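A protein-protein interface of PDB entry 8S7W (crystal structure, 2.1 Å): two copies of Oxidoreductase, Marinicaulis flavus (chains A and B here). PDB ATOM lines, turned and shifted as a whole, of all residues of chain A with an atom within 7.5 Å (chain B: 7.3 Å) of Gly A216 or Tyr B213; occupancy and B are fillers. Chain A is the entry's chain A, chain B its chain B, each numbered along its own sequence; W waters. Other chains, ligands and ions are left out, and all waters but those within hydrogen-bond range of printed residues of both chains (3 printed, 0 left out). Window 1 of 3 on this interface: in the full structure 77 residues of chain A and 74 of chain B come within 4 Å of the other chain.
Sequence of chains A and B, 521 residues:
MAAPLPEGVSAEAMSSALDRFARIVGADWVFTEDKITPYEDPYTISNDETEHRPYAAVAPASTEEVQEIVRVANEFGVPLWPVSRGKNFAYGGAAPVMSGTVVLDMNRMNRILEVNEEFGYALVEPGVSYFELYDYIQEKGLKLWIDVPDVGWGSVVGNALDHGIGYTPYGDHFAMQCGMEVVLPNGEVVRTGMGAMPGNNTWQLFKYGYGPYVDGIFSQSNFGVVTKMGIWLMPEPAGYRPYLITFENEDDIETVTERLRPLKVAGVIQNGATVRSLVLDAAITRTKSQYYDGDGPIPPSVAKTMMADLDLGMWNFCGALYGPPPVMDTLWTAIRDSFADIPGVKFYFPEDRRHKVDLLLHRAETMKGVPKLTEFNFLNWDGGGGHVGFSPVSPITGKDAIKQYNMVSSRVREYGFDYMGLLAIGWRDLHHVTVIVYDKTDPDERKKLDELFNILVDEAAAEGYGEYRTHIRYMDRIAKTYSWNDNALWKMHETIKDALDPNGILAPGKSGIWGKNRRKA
O of Gln A220 sits close to N of Pro B212 (3.4 Å).
The backbone carbonyl oxygen of Tyr A213 lies within hydrogen-bond range of the backbone NH of Ile B217, 3.3 Å away.
The backbone carbonyl oxygen (O) of Tyr B213 lies within hydrogen-bond range of the backbone NH (N) of Ile A217, 3.2 Å away.
The backbone carbonyl oxygen (O) of Gly A216 is in hydrogen-bond range of the backbone NH (N) of Tyr B213, at 3.0 Å.
The backbone NH (N) of Gly B211 lies within hydrogen-bond range of the side-chain amide oxygen (OE1) of Gln A220, 3.0 Å away.
The backbone carbonyl oxygen of Gly B216 is in hydrogen-bond range of the backbone NH of Tyr A213 (3.1 Å).
The side-chain hydroxyl of Tyr B208 lies within hydrogen-bond range of the backbone NH of Ala A175, at 3.2 Å.
N of Phe A223 sits at hydrogen-bond distance from OG of Ser A221, at 3.0 Å.
A ring nitrogen (NE2) of His A163 is in hydrogen-bond range of the side-chain hydroxyl of Ser A219 (2.8 Å).
NZ of Lys B207 lies within hydrogen-bond range of OH of Tyr B213 (3.4 Å).
Among the printed residues, merely in contact across the chains: Ser A219 with Pro B212, Phe A174 with Tyr B208, Ile A217 with Ile B217, His A163 with Gly B211, His A493 with Val B214, His A493 with Pro B212, His A163 with Tyr B208, Gln A220 with Tyr B210, Ile A217 with Pro B212, Ser A219 with Tyr B213 and Phe A223 with Pro B212.
Of the printed residues of chain B, His A163 touches Tyr B208 and Gly B211.
Gly A216 touches just one residue of chain B: Tyr B213 (3.0 Å).
Lys B207 touches none of the printed residues of chain A.
Printed residues of chain A within 4 Å of Gly B211: His A163 and Gln A220.
Tyr B213 touches just these residues of chain A: Gly A216 (3.0 Å), Ile A217 (3.2 Å) and Ser A219 (3.9 Å).
The nearest residue of chain B that does not touch Gly A216 is Pro B212 (4.05 Å).
The nearest printed residue of chain A that does not touch Tyr B210 is His A493 (4.6 Å).
Hydrophobic or aromatic side chains of chain A that line the printed part of chain B: His A163, Phe A174, Ala A175, Tyr A213, Ile A217, Phe A223 and His A493.
Along chain A the printed residues that touch a printed residue of chain B span positions 163 to 493.
Of the 19 printed residues of chain B, 8 touch a printed residue of chain A.
Hydrophobic or aromatic side chains of chain B within 4 Å of the printed part of chain A: Tyr B208, Tyr B210, Pro B212, Tyr B213, Val B214 and Ile B217.
Tyr A213 touches Gly B216, and with the chains exchanged Gly A216 touches Tyr B213.
Tyr A213 touches Ile B217, and with the chains exchanged Ile A217 touches Tyr B213.
Ile B217 touches its own counterpart, Ile A217.
Water W2 lies within hydrogen-bond range of O of Tyr B210 (2.5 Å), O of Pro B212 (2.7 Å) and NE2 of His A493 (2.9 Å).
Water W1 lies within hydrogen-bond range of a ring nitrogen (ND1) of His A163, the backbone carbonyl oxygen (O) of Gly B209 and the side-chain amide oxygen (OE1) of Gln A220.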
ATOM      1  N   LEU A 161     -11.173  26.642  31.283  1.00  0.00           N
ATOM      2  CA  LEU A 161     -10.863  27.210  29.946  1.00  0.00           C
ATOM      3  C   LEU A 161      -9.442  27.774  29.922  1.00  0.00           C
ATOM      4  O   LEU A 161      -8.809  27.672  28.869  1.00  0.00           O
ATOM      5  CB  LEU A 161     -11.873  28.300  29.587  1.00  0.00           C
ATOM      6  CG  LEU A 161     -13.307  27.803  29.408  1.00  0.00           C
ATOM      7  CD1 LEU A 161     -14.236  28.964  29.169  1.00  0.00           C
ATOM      8  CD2 LEU A 161     -13.393  26.794  28.271  1.00  0.00           C
ATOM      9  N   HIS A 163      -6.958  26.331  31.293  1.00  0.00           N
ATOM     10  CA  HIS A 163      -6.138  25.095  31.530  1.00  0.00           C
ATOM     11  C   HIS A 163      -5.660  25.063  32.985  1.00  0.00           C
ATOM     12  O   HIS A 163      -4.470  24.757  33.231  1.00  0.00           O
ATOM     13  CB  HIS A 163      -4.988  24.959  30.530  1.00  0.00           C
ATOM     14  CG  HIS A 163      -5.405  24.907  29.094  1.00  0.00           C
ATOM     15  ND1 HIS A 163      -4.496  25.082  28.054  1.00  0.00           N
ATOM     16  CD2 HIS A 163      -6.613  24.719  28.511  1.00  0.00           C
ATOM     17  CE1 HIS A 163      -5.143  25.024  26.911  1.00  0.00           C
ATOM     18  NE2 HIS A 163      -6.433  24.822  27.153  1.00  0.00           N
ATOM     19  N   PHE A 174      -9.469  21.031  32.417  1.00  0.00           N
ATOM     20  CA  PHE A 174      -9.979  21.016  31.018  1.00  0.00           C
ATOM     21  C   PHE A 174     -10.106  19.565  30.512  1.00  0.00           C
ATOM     22  O   PHE A 174     -11.039  19.300  29.714  1.00  0.00           O
ATOM     23  CB  PHE A 174      -9.167  21.912  30.078  1.00  0.00           C
ATOM     24  CG  PHE A 174      -9.962  22.202  28.842  1.00  0.00           C
ATOM     25  CD1 PHE A 174     -11.132  22.944  28.933  1.00  0.00           C
ATOM     26  CD2 PHE A 174      -9.680  21.559  27.648  1.00  0.00           C
ATOM     27  CE1 PHE A 174     -11.960  23.106  27.829  1.00  0.00           C
ATOM     28  CE2 PHE A 174     -10.495  21.734  26.540  1.00  0.00           C
ATOM     29  CZ  PHE A 174     -11.633  22.505  26.630  1.00  0.00           C
ATOM     30  N   ALA A 175      -9.247  18.626  30.954  1.00  0.00           N
ATOM     31  CA  ALA A 175      -9.324  17.216  30.524  1.00  0.00           C
ATOM     32  C   ALA A 175     -10.630  16.610  31.039  1.00  0.00           C
ATOM     33  O   ALA A 175     -11.098  15.666  30.406  1.00  0.00           O
ATOM     34  CB  ALA A 175      -8.138  16.431  30.998  1.00  0.00           C
ATOM     35  N   GLN A 177     -13.478  18.288  31.272  1.00  0.00           N
ATOM     36  CA  GLN A 177     -14.598  18.997  30.580  1.00  0.00           C
ATOM     37  C   GLN A 177     -15.295  18.056  29.584  1.00  0.00           C
ATOM     38  O   GLN A 177     -14.638  17.182  28.996  1.00  0.00           O
ATOM     39  CB  GLN A 177     -14.104  20.281  29.896  1.00  0.00           C
ATOM     40  CG  GLN A 177     -15.146  21.041  29.098  1.00  0.00           C
ATOM     41  CD  GLN A 177     -15.209  20.595  27.660  1.00  0.00           C
ATOM     42  OE1 GLN A 177     -14.281  19.983  27.126  1.00  0.00           O
ATOM     43  NE2 GLN A 177     -16.330  20.870  27.010  1.00  0.00           N
ATOM     44  N   MET A 180     -19.940  21.692  25.783  1.00  0.00           N
ATOM     45  CA  MET A 180     -20.058  23.139  26.073  1.00  0.00           C
ATOM     46  C   MET A 180     -21.042  23.785  25.095  1.00  0.00           C
ATOM     47  O   MET A 180     -21.290  23.232  24.022  1.00  0.00           O
ATOM     48  CB  MET A 180     -18.691  23.834  26.035  1.00  0.00           C
ATOM     49  CG  MET A 180     -17.982  23.692  24.721  1.00  0.00           C
ATOM     50  SD  MET A 180     -16.526  24.806  24.607  1.00  0.00           S
ATOM     51  CE  MET A 180     -15.523  24.165  25.946  1.00  0.00           C
ATOM     52  N   THR A 192     -21.392  21.661  21.473  1.00  0.00           N
ATOM     53  CA  THR A 192     -20.414  20.622  21.057  1.00  0.00           C
ATOM     54  C   THR A 192     -20.898  19.229  21.487  1.00  0.00           C
ATOM     55  O   THR A 192     -21.785  19.157  22.378  1.00  0.00           O
ATOM     56  CB  THR A 192     -19.053  20.921  21.673  1.00  0.00           C
ATOM     57  OG1 THR A 192     -19.219  20.742  23.079  1.00  0.00           O
ATOM     58  CG2 THR A 192     -18.599  22.316  21.329  1.00  0.00           C
ATOM     59  N   TYR A 213     -13.309  17.295  16.718  1.00  0.00           N
ATOM     60  CA  TYR A 213     -13.371  17.524  18.179  1.00  0.00           C
ATOM     61  C   TYR A 213     -12.930  18.970  18.420  1.00  0.00           C
ATOM     62  O   TYR A 213     -11.734  19.251  18.286  1.00  0.00           O
ATOM     63  CB  TYR A 213     -12.551  16.429  18.877  1.00  0.00           C
ATOM     64  CG  TYR A 213     -12.554  16.539  20.377  1.00  0.00           C
ATOM     65  CD1 TYR A 213     -13.676  17.006  21.051  1.00  0.00           C
ATOM     66  CD2 TYR A 213     -11.450  16.148  21.131  1.00  0.00           C
ATOM     67  CE1 TYR A 213     -13.697  17.125  22.428  1.00  0.00           C
ATOM     68  CE2 TYR A 213     -11.465  16.228  22.519  1.00  0.00           C
ATOM     69  CZ  TYR A 213     -12.591  16.738  23.168  1.00  0.00           C
ATOM     70  OH  TYR A 213     -12.633  16.875  24.525  1.00  0.00           O
ATOM     71  N   VAL A 214     -13.869  19.878  18.700  1.00  0.00           N
ATOM     72  CA  VAL A 214     -13.608  21.351  18.644  1.00  0.00           C
ATOM     73  C   VAL A 214     -13.623  22.004  20.030  1.00  0.00           C
ATOM     74  O   VAL A 214     -13.226  23.183  20.089  1.00  0.00           O
ATOM     75  CB  VAL A 214     -14.576  22.062  17.673  1.00  0.00           C
ATOM     76  CG1 VAL A 214     -14.336  21.615  16.221  1.00  0.00           C
ATOM     77  CG2 VAL A 214     -16.023  21.885  18.084  1.00  0.00           C
ATOM     78  N   ASP A 215     -14.004  21.294  21.105  1.00  0.00           N
ATOM     79  CA  ASP A 215     -14.165  21.920  22.449  1.00  0.00           C
ATOM     80  C   ASP A 215     -12.881  22.690  22.787  1.00  0.00           C
ATOM     81  O   ASP A 215     -12.960  23.797  23.361  1.00  0.00           O
ATOM     82  CB  ASP A 215     -14.493  20.887  23.542  1.00  0.00           C
ATOM     83  CG  ASP A 215     -15.864  20.241  23.380  1.00  0.00           C
ATOM     84  OD1 ASP A 215     -16.059  19.541  22.372  1.00  0.00           O
ATOM     85  OD2 ASP A 215     -16.736  20.459  24.252  1.00  0.00           O
ATOM     86  N   GLY A 216     -11.746  22.061  22.503  1.00  0.00           N
ATOM     87  CA  GLY A 216     -10.408  22.586  22.807  1.00  0.00           C
ATOM     88  C   GLY A 216     -10.144  23.969  22.235  1.00  0.00           C
ATOM     89  O   GLY A 216      -9.387  24.697  22.863  1.00  0.00           O
ATOM     90  N   ILE A 217     -10.712  24.306  21.083  1.00  0.00           N
ATOM     91  CA  ILE A 217     -10.407  25.585  20.395  1.00  0.00           C
ATOM     92  C   ILE A 217     -11.025  26.745  21.177  1.00  0.00           C
ATOM     93  O   ILE A 217     -10.621  27.888  20.895  1.00  0.00           O
ATOM     94  CB  ILE A 217     -10.804  25.608  18.907  1.00  0.00           C
ATOM     95  CG1 ILE A 217     -12.263  25.996  18.659  1.00  0.00           C
ATOM     96  CG2 ILE A 217     -10.439  24.322  18.212  1.00  0.00           C
ATOM     97  CD1 ILE A 217     -12.634  25.927  17.169  1.00  0.00           C
ATOM     98  N   PHE A 218     -11.918  26.487  22.138  1.00  0.00           N
ATOM     99  CA  PHE A 218     -12.522  27.581  22.934  1.00  0.00           C
ATOM    100  C   PHE A 218     -11.853  27.684  24.299  1.00  0.00           C
ATOM    101  O   PHE A 218     -12.368  28.475  25.143  1.00  0.00           O
ATOM    102  CB  PHE A 218     -14.031  27.374  23.026  1.00  0.00           C
ATOM    103  CG  PHE A 218     -14.684  27.368  21.674  1.00  0.00           C
ATOM    104  CD1 PHE A 218     -14.806  28.539  20.950  1.00  0.00           C
ATOM    105  CD2 PHE A 218     -15.148  26.196  21.106  1.00  0.00           C
ATOM    106  CE1 PHE A 218     -15.386  28.541  19.691  1.00  0.00           C
ATOM    107  CE2 PHE A 218     -15.745  26.200  19.857  1.00  0.00           C
ATOM    108  CZ  PHE A 218     -15.855  27.374  19.139  1.00  0.00           C
ATOM    109  N   SER A 219     -10.800  26.898  24.542  1.00  0.00           N
ATOM    110  CA  SER A 219      -9.925  27.031  25.734  1.00  0.00           C
ATOM    111  C   SER A 219      -8.720  27.918  25.374  1.00  0.00           C
ATOM    112  O   SER A 219      -8.274  27.890  24.201  1.00  0.00           O
ATOM    113  CB  SER A 219      -9.517  25.668  26.282  1.00  0.00           C
ATOM    114  OG  SER A 219      -8.608  25.003  25.397  1.00  0.00           O
ATOM    115  N   GLN A 220      -8.248  28.730  26.332  1.00  0.00           N
ATOM    116  CA  GLN A 220      -7.170  29.748  26.168  1.00  0.00           C
ATOM    117  C   GLN A 220      -7.323  30.457  24.823  1.00  0.00           C
ATOM    118  O   GLN A 220      -6.325  30.531  24.041  1.00  0.00           O
ATOM    119  CB  GLN A 220      -5.797  29.101  26.312  1.00  0.00           C
ATOM    120  CG  GLN A 220      -5.476  28.711  27.755  1.00  0.00           C
ATOM    121  CD  GLN A 220      -3.996  28.526  28.028  1.00  0.00           C
ATOM    122  OE1 GLN A 220      -3.150  28.546  27.127  1.00  0.00           O
ATOM    123  NE2 GLN A 220      -3.655  28.356  29.294  1.00  0.00           N
ATOM    124  N   SER A 221      -8.532  30.965  24.562  1.00  0.00           N
ATOM    125  CA  SER A 221      -8.989  31.273  23.187  1.00  0.00           C
ATOM    126  C   SER A 221      -9.787  32.573  23.144  1.00  0.00           C
ATOM    127  O   SER A 221     -10.342  33.009  24.160  1.00  0.00           O
ATOM    128  CB  SER A 221      -9.820  30.121  22.647  1.00  0.00           C
ATOM    129  OG  SER A 221     -10.310  30.412  21.355  1.00  0.00           O
ATOM    130  N   PHE A 223     -11.950  32.668  20.321  1.00  0.00           N
ATOM    131  CA  PHE A 223     -12.800  32.162  19.216  1.00  0.00           C
ATOM    132  C   PHE A 223     -14.278  32.103  19.616  1.00  0.00           C
ATOM    133  O   PHE A 223     -15.077  31.903  18.704  1.00  0.00           O
ATOM    134  CB  PHE A 223     -12.373  30.774  18.746  1.00  0.00           C
ATOM    135  CG  PHE A 223     -10.992  30.694  18.179  1.00  0.00           C
ATOM    136  CD1 PHE A 223     -10.305  31.836  17.784  1.00  0.00           C
ATOM    137  CD2 PHE A 223     -10.339  29.479  18.122  1.00  0.00           C
ATOM    138  CE1 PHE A 223      -9.022  31.747  17.274  1.00  0.00           C
ATOM    139  CE2 PHE A 223      -9.051  29.399  17.619  1.00  0.00           C
ATOM    140  CZ  PHE A 223      -8.395  30.530  17.186  1.00  0.00           C
ATOM    141  N   HIS A 493      -3.847  29.740  13.888  1.00  0.00           N
ATOM    142  CA  HIS A 493      -4.776  30.357  14.867  1.00  0.00           C
ATOM    143  C   HIS A 493      -5.341  31.642  14.271  1.00  0.00           C
ATOM    144  O   HIS A 493      -6.520  31.879  14.462  1.00  0.00           O
ATOM    145  CB  HIS A 493      -4.094  30.686  16.200  1.00  0.00           C
ATOM    146  CG  HIS A 493      -3.727  29.508  17.024  1.00  0.00           C
ATOM    147  ND1 HIS A 493      -4.432  28.343  16.991  1.00  0.00           N
ATOM    148  CD2 HIS A 493      -2.717  29.318  17.885  1.00  0.00           C
ATOM    149  CE1 HIS A 493      -3.888  27.472  17.802  1.00  0.00           C
ATOM    150  NE2 HIS A 493      -2.830  28.053  18.378  1.00  0.00           N
ATOM    151  N   PHE B 174      -7.592   8.168  20.648  1.00  0.00           N
ATOM    152  CA  PHE B 174      -7.396   9.624  20.463  1.00  0.00           C
ATOM    153  C   PHE B 174      -7.162  10.346  21.805  1.00  0.00           C
ATOM    154  O   PHE B 174      -6.416  11.366  21.822  1.00  0.00           O
ATOM    155  CB  PHE B 174      -8.495  10.255  19.612  1.00  0.00           C
ATOM    156  CG  PHE B 174      -8.092  11.648  19.170  1.00  0.00           C
ATOM    157  CD1 PHE B 174      -7.067  11.826  18.246  1.00  0.00           C
ATOM    158  CD2 PHE B 174      -8.662  12.776  19.753  1.00  0.00           C
ATOM    159  CE1 PHE B 174      -6.687  13.099  17.840  1.00  0.00           C
ATOM    160  CE2 PHE B 174      -8.276  14.044  19.351  1.00  0.00           C
ATOM    161  CZ  PHE B 174      -7.300  14.206  18.391  1.00  0.00           C
ATOM    162  N   ALA B 175      -7.668   9.830  22.927  1.00  0.00           N
ATOM    163  CA  ALA B 175      -7.402  10.425  24.253  1.00  0.00           C
ATOM    164  C   ALA B 175      -5.920  10.267  24.594  1.00  0.00           C
ATOM    165  O   ALA B 175      -5.364  11.132  25.339  1.00  0.00           O
ATOM    166  CB  ALA B 175      -8.311   9.842  25.297  1.00  0.00           C
ATOM    167  N   GLN B 177      -3.497  10.343  22.375  1.00  0.00           N
ATOM    168  CA  GLN B 177      -2.709  11.128  21.378  1.00  0.00           C
ATOM    169  C   GLN B 177      -2.079  12.370  22.053  1.00  0.00           C
ATOM    170  O   GLN B 177      -2.683  12.987  22.984  1.00  0.00           O
ATOM    171  CB  GLN B 177      -3.568  11.490  20.156  1.00  0.00           C
ATOM    172  CG  GLN B 177      -2.833  12.357  19.130  1.00  0.00           C
ATOM    173  CD  GLN B 177      -2.935  13.832  19.457  1.00  0.00           C
ATOM    174  OE1 GLN B 177      -3.877  14.276  20.081  1.00  0.00           O
ATOM    175  NE2 GLN B 177      -1.990  14.621  18.990  1.00  0.00           N
ATOM    176  N   CYS B 178      -0.845  12.699  21.666  1.00  0.00           N
ATOM    177  CA  CYS B 178      -0.092  13.835  22.252  1.00  0.00           C
ATOM    178  C   CYS B 178       0.923  14.340  21.216  1.00  0.00           C
ATOM    179  O   CYS B 178       1.901  13.652  20.949  1.00  0.00           O
ATOM    180  CB  CYS B 178       0.547  13.425  23.563  1.00  0.00           C
ATOM    181  SG  CYS B 178       1.268  14.792  24.502  1.00  0.00           S
ATOM    182  N   GLY B 179       0.646  15.504  20.646  1.00  0.00           N
ATOM    183  CA  GLY B 179       1.458  16.127  19.594  1.00  0.00           C
ATOM    184  C   GLY B 179       1.140  15.544  18.234  1.00  0.00           C
ATOM    185  O   GLY B 179       0.987  14.318  18.137  1.00  0.00           O
ATOM    186  N   THR B 192       1.582  20.868  16.529  1.00  0.00           N
ATOM    187  CA  THR B 192       0.678  21.231  17.654  1.00  0.00           C
ATOM    188  C   THR B 192       1.428  21.099  18.974  1.00  0.00           C
ATOM    189  O   THR B 192       2.446  20.382  19.028  1.00  0.00           O
ATOM    190  CB  THR B 192      -0.566  20.340  17.699  1.00  0.00           C
ATOM    191  OG1 THR B 192      -0.112  19.029  18.035  1.00  0.00           O
ATOM    192  CG2 THR B 192      -1.325  20.364  16.393  1.00  0.00           C
ATOM    193  N   GLY B 193       0.907  21.733  20.017  1.00  0.00           N
ATOM    194  CA  GLY B 193       1.429  21.558  21.384  1.00  0.00           C
ATOM    195  C   GLY B 193       2.870  22.016  21.535  1.00  0.00           C
ATOM    196  O   GLY B 193       3.257  23.066  20.967  1.00  0.00           O
ATOM    197  N   PHE B 206       3.083  16.562  26.998  1.00  0.00           N
ATOM    198  CA  PHE B 206       2.100  17.580  27.462  1.00  0.00           C
ATOM    199  C   PHE B 206       1.203  17.927  26.278  1.00  0.00           C
ATOM    200  O   PHE B 206       1.715  18.367  25.230  1.00  0.00           O
ATOM    201  CB  PHE B 206       2.846  18.777  28.069  1.00  0.00           C
ATOM    202  CG  PHE B 206       1.953  19.852  28.646  1.00  0.00           C
ATOM    203  CD1 PHE B 206       1.314  19.661  29.861  1.00  0.00           C
ATOM    204  CD2 PHE B 206       1.757  21.058  27.984  1.00  0.00           C
ATOM    205  CE1 PHE B 206       0.505  20.650  30.405  1.00  0.00           C
ATOM    206  CE2 PHE B 206       0.964  22.054  28.538  1.00  0.00           C
ATOM    207  CZ  PHE B 206       0.324  21.846  29.742  1.00  0.00           C
ATOM    208  N   LYS B 207      -0.092  17.691  26.389  1.00  0.00           N
ATOM    209  CA  LYS B 207      -0.965  17.793  25.188  1.00  0.00           C
ATOM    210  C   LYS B 207      -1.137  19.242  24.738  1.00  0.00           C
ATOM    211  O   LYS B 207      -1.108  19.474  23.512  1.00  0.00           O
ATOM    212  CB  LYS B 207      -2.346  17.195  25.440  1.00  0.00           C
ATOM    213  CG  LYS B 207      -2.410  15.670  25.515  1.00  0.00           C
ATOM    214  CD  LYS B 207      -3.736  15.275  26.141  1.00  0.00           C
ATOM    215  CE  LYS B 207      -4.274  13.930  25.747  1.00  0.00           C
ATOM    216  NZ  LYS B 207      -4.865  13.936  24.398  1.00  0.00           N
ATOM    217  N   TYR B 208      -1.371  20.178  25.667  1.00  0.00           N
ATOM    218  CA  TYR B 208      -1.967  21.498  25.316  1.00  0.00           C
ATOM    219  C   TYR B 208      -0.970  22.378  24.539  1.00  0.00           C
ATOM    220  O   TYR B 208      -1.401  23.077  23.610  1.00  0.00           O
ATOM    221  CB  TYR B 208      -2.478  22.265  26.546  1.00  0.00           C
ATOM    222  CG  TYR B 208      -3.576  21.592  27.329  1.00  0.00           C
ATOM    223  CD1 TYR B 208      -4.647  20.981  26.704  1.00  0.00           C
ATOM    224  CD2 TYR B 208      -3.517  21.524  28.715  1.00  0.00           C
ATOM    225  CE1 TYR B 208      -5.637  20.348  27.443  1.00  0.00           C
ATOM    226  CE2 TYR B 208      -4.495  20.888  29.468  1.00  0.00           C
ATOM    227  CZ  TYR B 208      -5.577  20.326  28.830  1.00  0.00           C
ATOM    228  OH  TYR B 208      -6.527  19.680  29.568  1.00  0.00           O
ATOM    229  N   GLY B 209       0.302  22.384  24.926  1.00  0.00           N
ATOM    230  CA  GLY B 209       1.153  23.554  24.654  1.00  0.00           C
ATOM    231  C   GLY B 209       0.487  24.799  25.194  1.00  0.00           C
ATOM    232  O   GLY B 209       0.080  24.784  26.374  1.00  0.00           O
ATOM    233  N   TYR B 210       0.379  25.837  24.370  1.00  0.00           N
ATOM    234  CA  TYR B 210      -0.096  27.175  24.759  1.00  0.00           C
ATOM    235  C   TYR B 210      -1.167  27.592  23.765  1.00  0.00           C
ATOM    236  O   TYR B 210      -1.041  27.319  22.551  1.00  0.00           O
ATOM    237  CB  TYR B 210       1.075  28.169  24.816  1.00  0.00           C
ATOM    238  CG  TYR B 210       0.706  29.614  25.034  1.00  0.00           C
ATOM    239  CD1 TYR B 210       0.113  30.056  26.204  1.00  0.00           C
ATOM    240  CD2 TYR B 210       0.985  30.560  24.072  1.00  0.00           C
ATOM    241  CE1 TYR B 210      -0.203  31.394  26.408  1.00  0.00           C
ATOM    242  CE2 TYR B 210       0.719  31.902  24.270  1.00  0.00           C
ATOM    243  CZ  TYR B 210       0.133  32.324  25.447  1.00  0.00           C
ATOM    244  OH  TYR B 210      -0.151  33.640  25.588  1.00  0.00           O
ATOM    245  N   GLY B 211      -2.168  28.300  24.267  1.00  0.00           N
ATOM    246  CA  GLY B 211      -3.245  28.878  23.456  1.00  0.00           C
ATOM    247  C   GLY B 211      -4.279  27.792  23.157  1.00  0.00           C
ATOM    248  O   GLY B 211      -4.387  26.803  23.918  1.00  0.00           O
ATOM    249  N   PRO B 212      -5.100  27.971  22.098  1.00  0.00           N
ATOM    250  CA  PRO B 212      -6.176  27.034  21.798  1.00  0.00           C
ATOM    251  C   PRO B 212      -5.674  25.604  21.530  1.00  0.00           C
ATOM    252  O   PRO B 212      -4.623  25.388  20.916  1.00  0.00           O
ATOM    253  CB  PRO B 212      -6.866  27.625  20.557  1.00  0.00           C
ATOM    254  CG  PRO B 212      -6.432  29.090  20.564  1.00  0.00           C
ATOM    255  CD  PRO B 212      -5.037  29.068  21.130  1.00  0.00           C
ATOM    256  N   TYR B 213      -6.480  24.641  21.968  1.00  0.00           N
ATOM    257  CA  TYR B 213      -6.186  23.204  21.851  1.00  0.00           C
ATOM    258  C   TYR B 213      -6.876  22.678  20.589  1.00  0.00           C
ATOM    259  O   TYR B 213      -8.119  22.558  20.560  1.00  0.00           O
ATOM    260  CB  TYR B 213      -6.595  22.524  23.156  1.00  0.00           C
ATOM    261  CG  TYR B 213      -6.289  21.061  23.146  1.00  0.00           C
ATOM    262  CD1 TYR B 213      -5.078  20.589  22.671  1.00  0.00           C
ATOM    263  CD2 TYR B 213      -7.197  20.151  23.636  1.00  0.00           C
ATOM    264  CE1 TYR B 213      -4.787  19.239  22.648  1.00  0.00           C
ATOM    265  CE2 TYR B 213      -6.924  18.794  23.633  1.00  0.00           C
ATOM    266  CZ  TYR B 213      -5.723  18.334  23.113  1.00  0.00           C
ATOM    267  OH  TYR B 213      -5.469  16.998  23.127  1.00  0.00           O
ATOM    268  N   VAL B 214      -6.078  22.398  19.560  1.00  0.00           N
ATOM    269  CA  VAL B 214      -6.533  22.269  18.152  1.00  0.00           C
ATOM    270  C   VAL B 214      -6.311  20.834  17.646  1.00  0.00           C
ATOM    271  O   VAL B 214      -6.798  20.539  16.551  1.00  0.00           O
ATOM    272  CB  VAL B 214      -5.852  23.303  17.223  1.00  0.00           C
ATOM    273  CG1 VAL B 214      -6.247  24.723  17.553  1.00  0.00           C
ATOM    274  CG2 VAL B 214      -4.340  23.190  17.180  1.00  0.00           C
ATOM    275  N   ASP B 215      -5.603  19.959  18.366  1.00  0.00           N
ATOM    276  CA  ASP B 215      -5.308  18.606  17.824  1.00  0.00           C
ATOM    277  C   ASP B 215      -6.616  17.919  17.418  1.00  0.00           C
ATOM    278  O   ASP B 215      -6.610  17.217  16.383  1.00  0.00           O
ATOM    279  CB  ASP B 215      -4.547  17.717  18.804  1.00  0.00           C
ATOM    280  CG  ASP B 215      -3.144  18.214  19.117  1.00  0.00           C
ATOM    281  OD1 ASP B 215      -3.046  19.329  19.677  1.00  0.00           O
ATOM    282  OD2 ASP B 215      -2.165  17.434  18.878  1.00  0.00           O
ATOM    283  N   GLY B 216      -7.679  18.111  18.214  1.00  0.00           N
ATOM    284  CA  GLY B 216      -8.996  17.481  18.022  1.00  0.00           C
ATOM    285  C   GLY B 216      -9.617  17.791  16.681  1.00  0.00           C
ATOM    286  O   GLY B 216     -10.298  16.909  16.161  1.00  0.00           O
ATOM    287  N   ILE B 217      -9.345  18.958  16.097  1.00  0.00           N
ATOM    288  CA  ILE B 217     -10.010  19.397  14.840  1.00  0.00           C
ATOM    289  C   ILE B 217      -9.469  18.604  13.649  1.00  0.00           C
ATOM    290  O   ILE B 217     -10.137  18.629  12.611  1.00  0.00           O
ATOM    291  CB  ILE B 217      -9.933  20.919  14.587  1.00  0.00           C
ATOM    292  CG1 ILE B 217      -8.617  21.351  13.926  1.00  0.00           C
ATOM    293  CG2 ILE B 217     -10.245  21.685  15.875  1.00  0.00           C
ATOM    294  CD1 ILE B 217      -8.579  22.824  13.528  1.00  0.00           C
HETATM  295  O   HOH W   1      -1.942  25.479  28.011  1.00  0.00           O
HETATM  296  O   HOH W   2      -2.046  26.225  20.519  1.00  0.00           O
HETATM  297  O   HOH W   3      -9.416  20.692  19.334  1.00  0.00           O
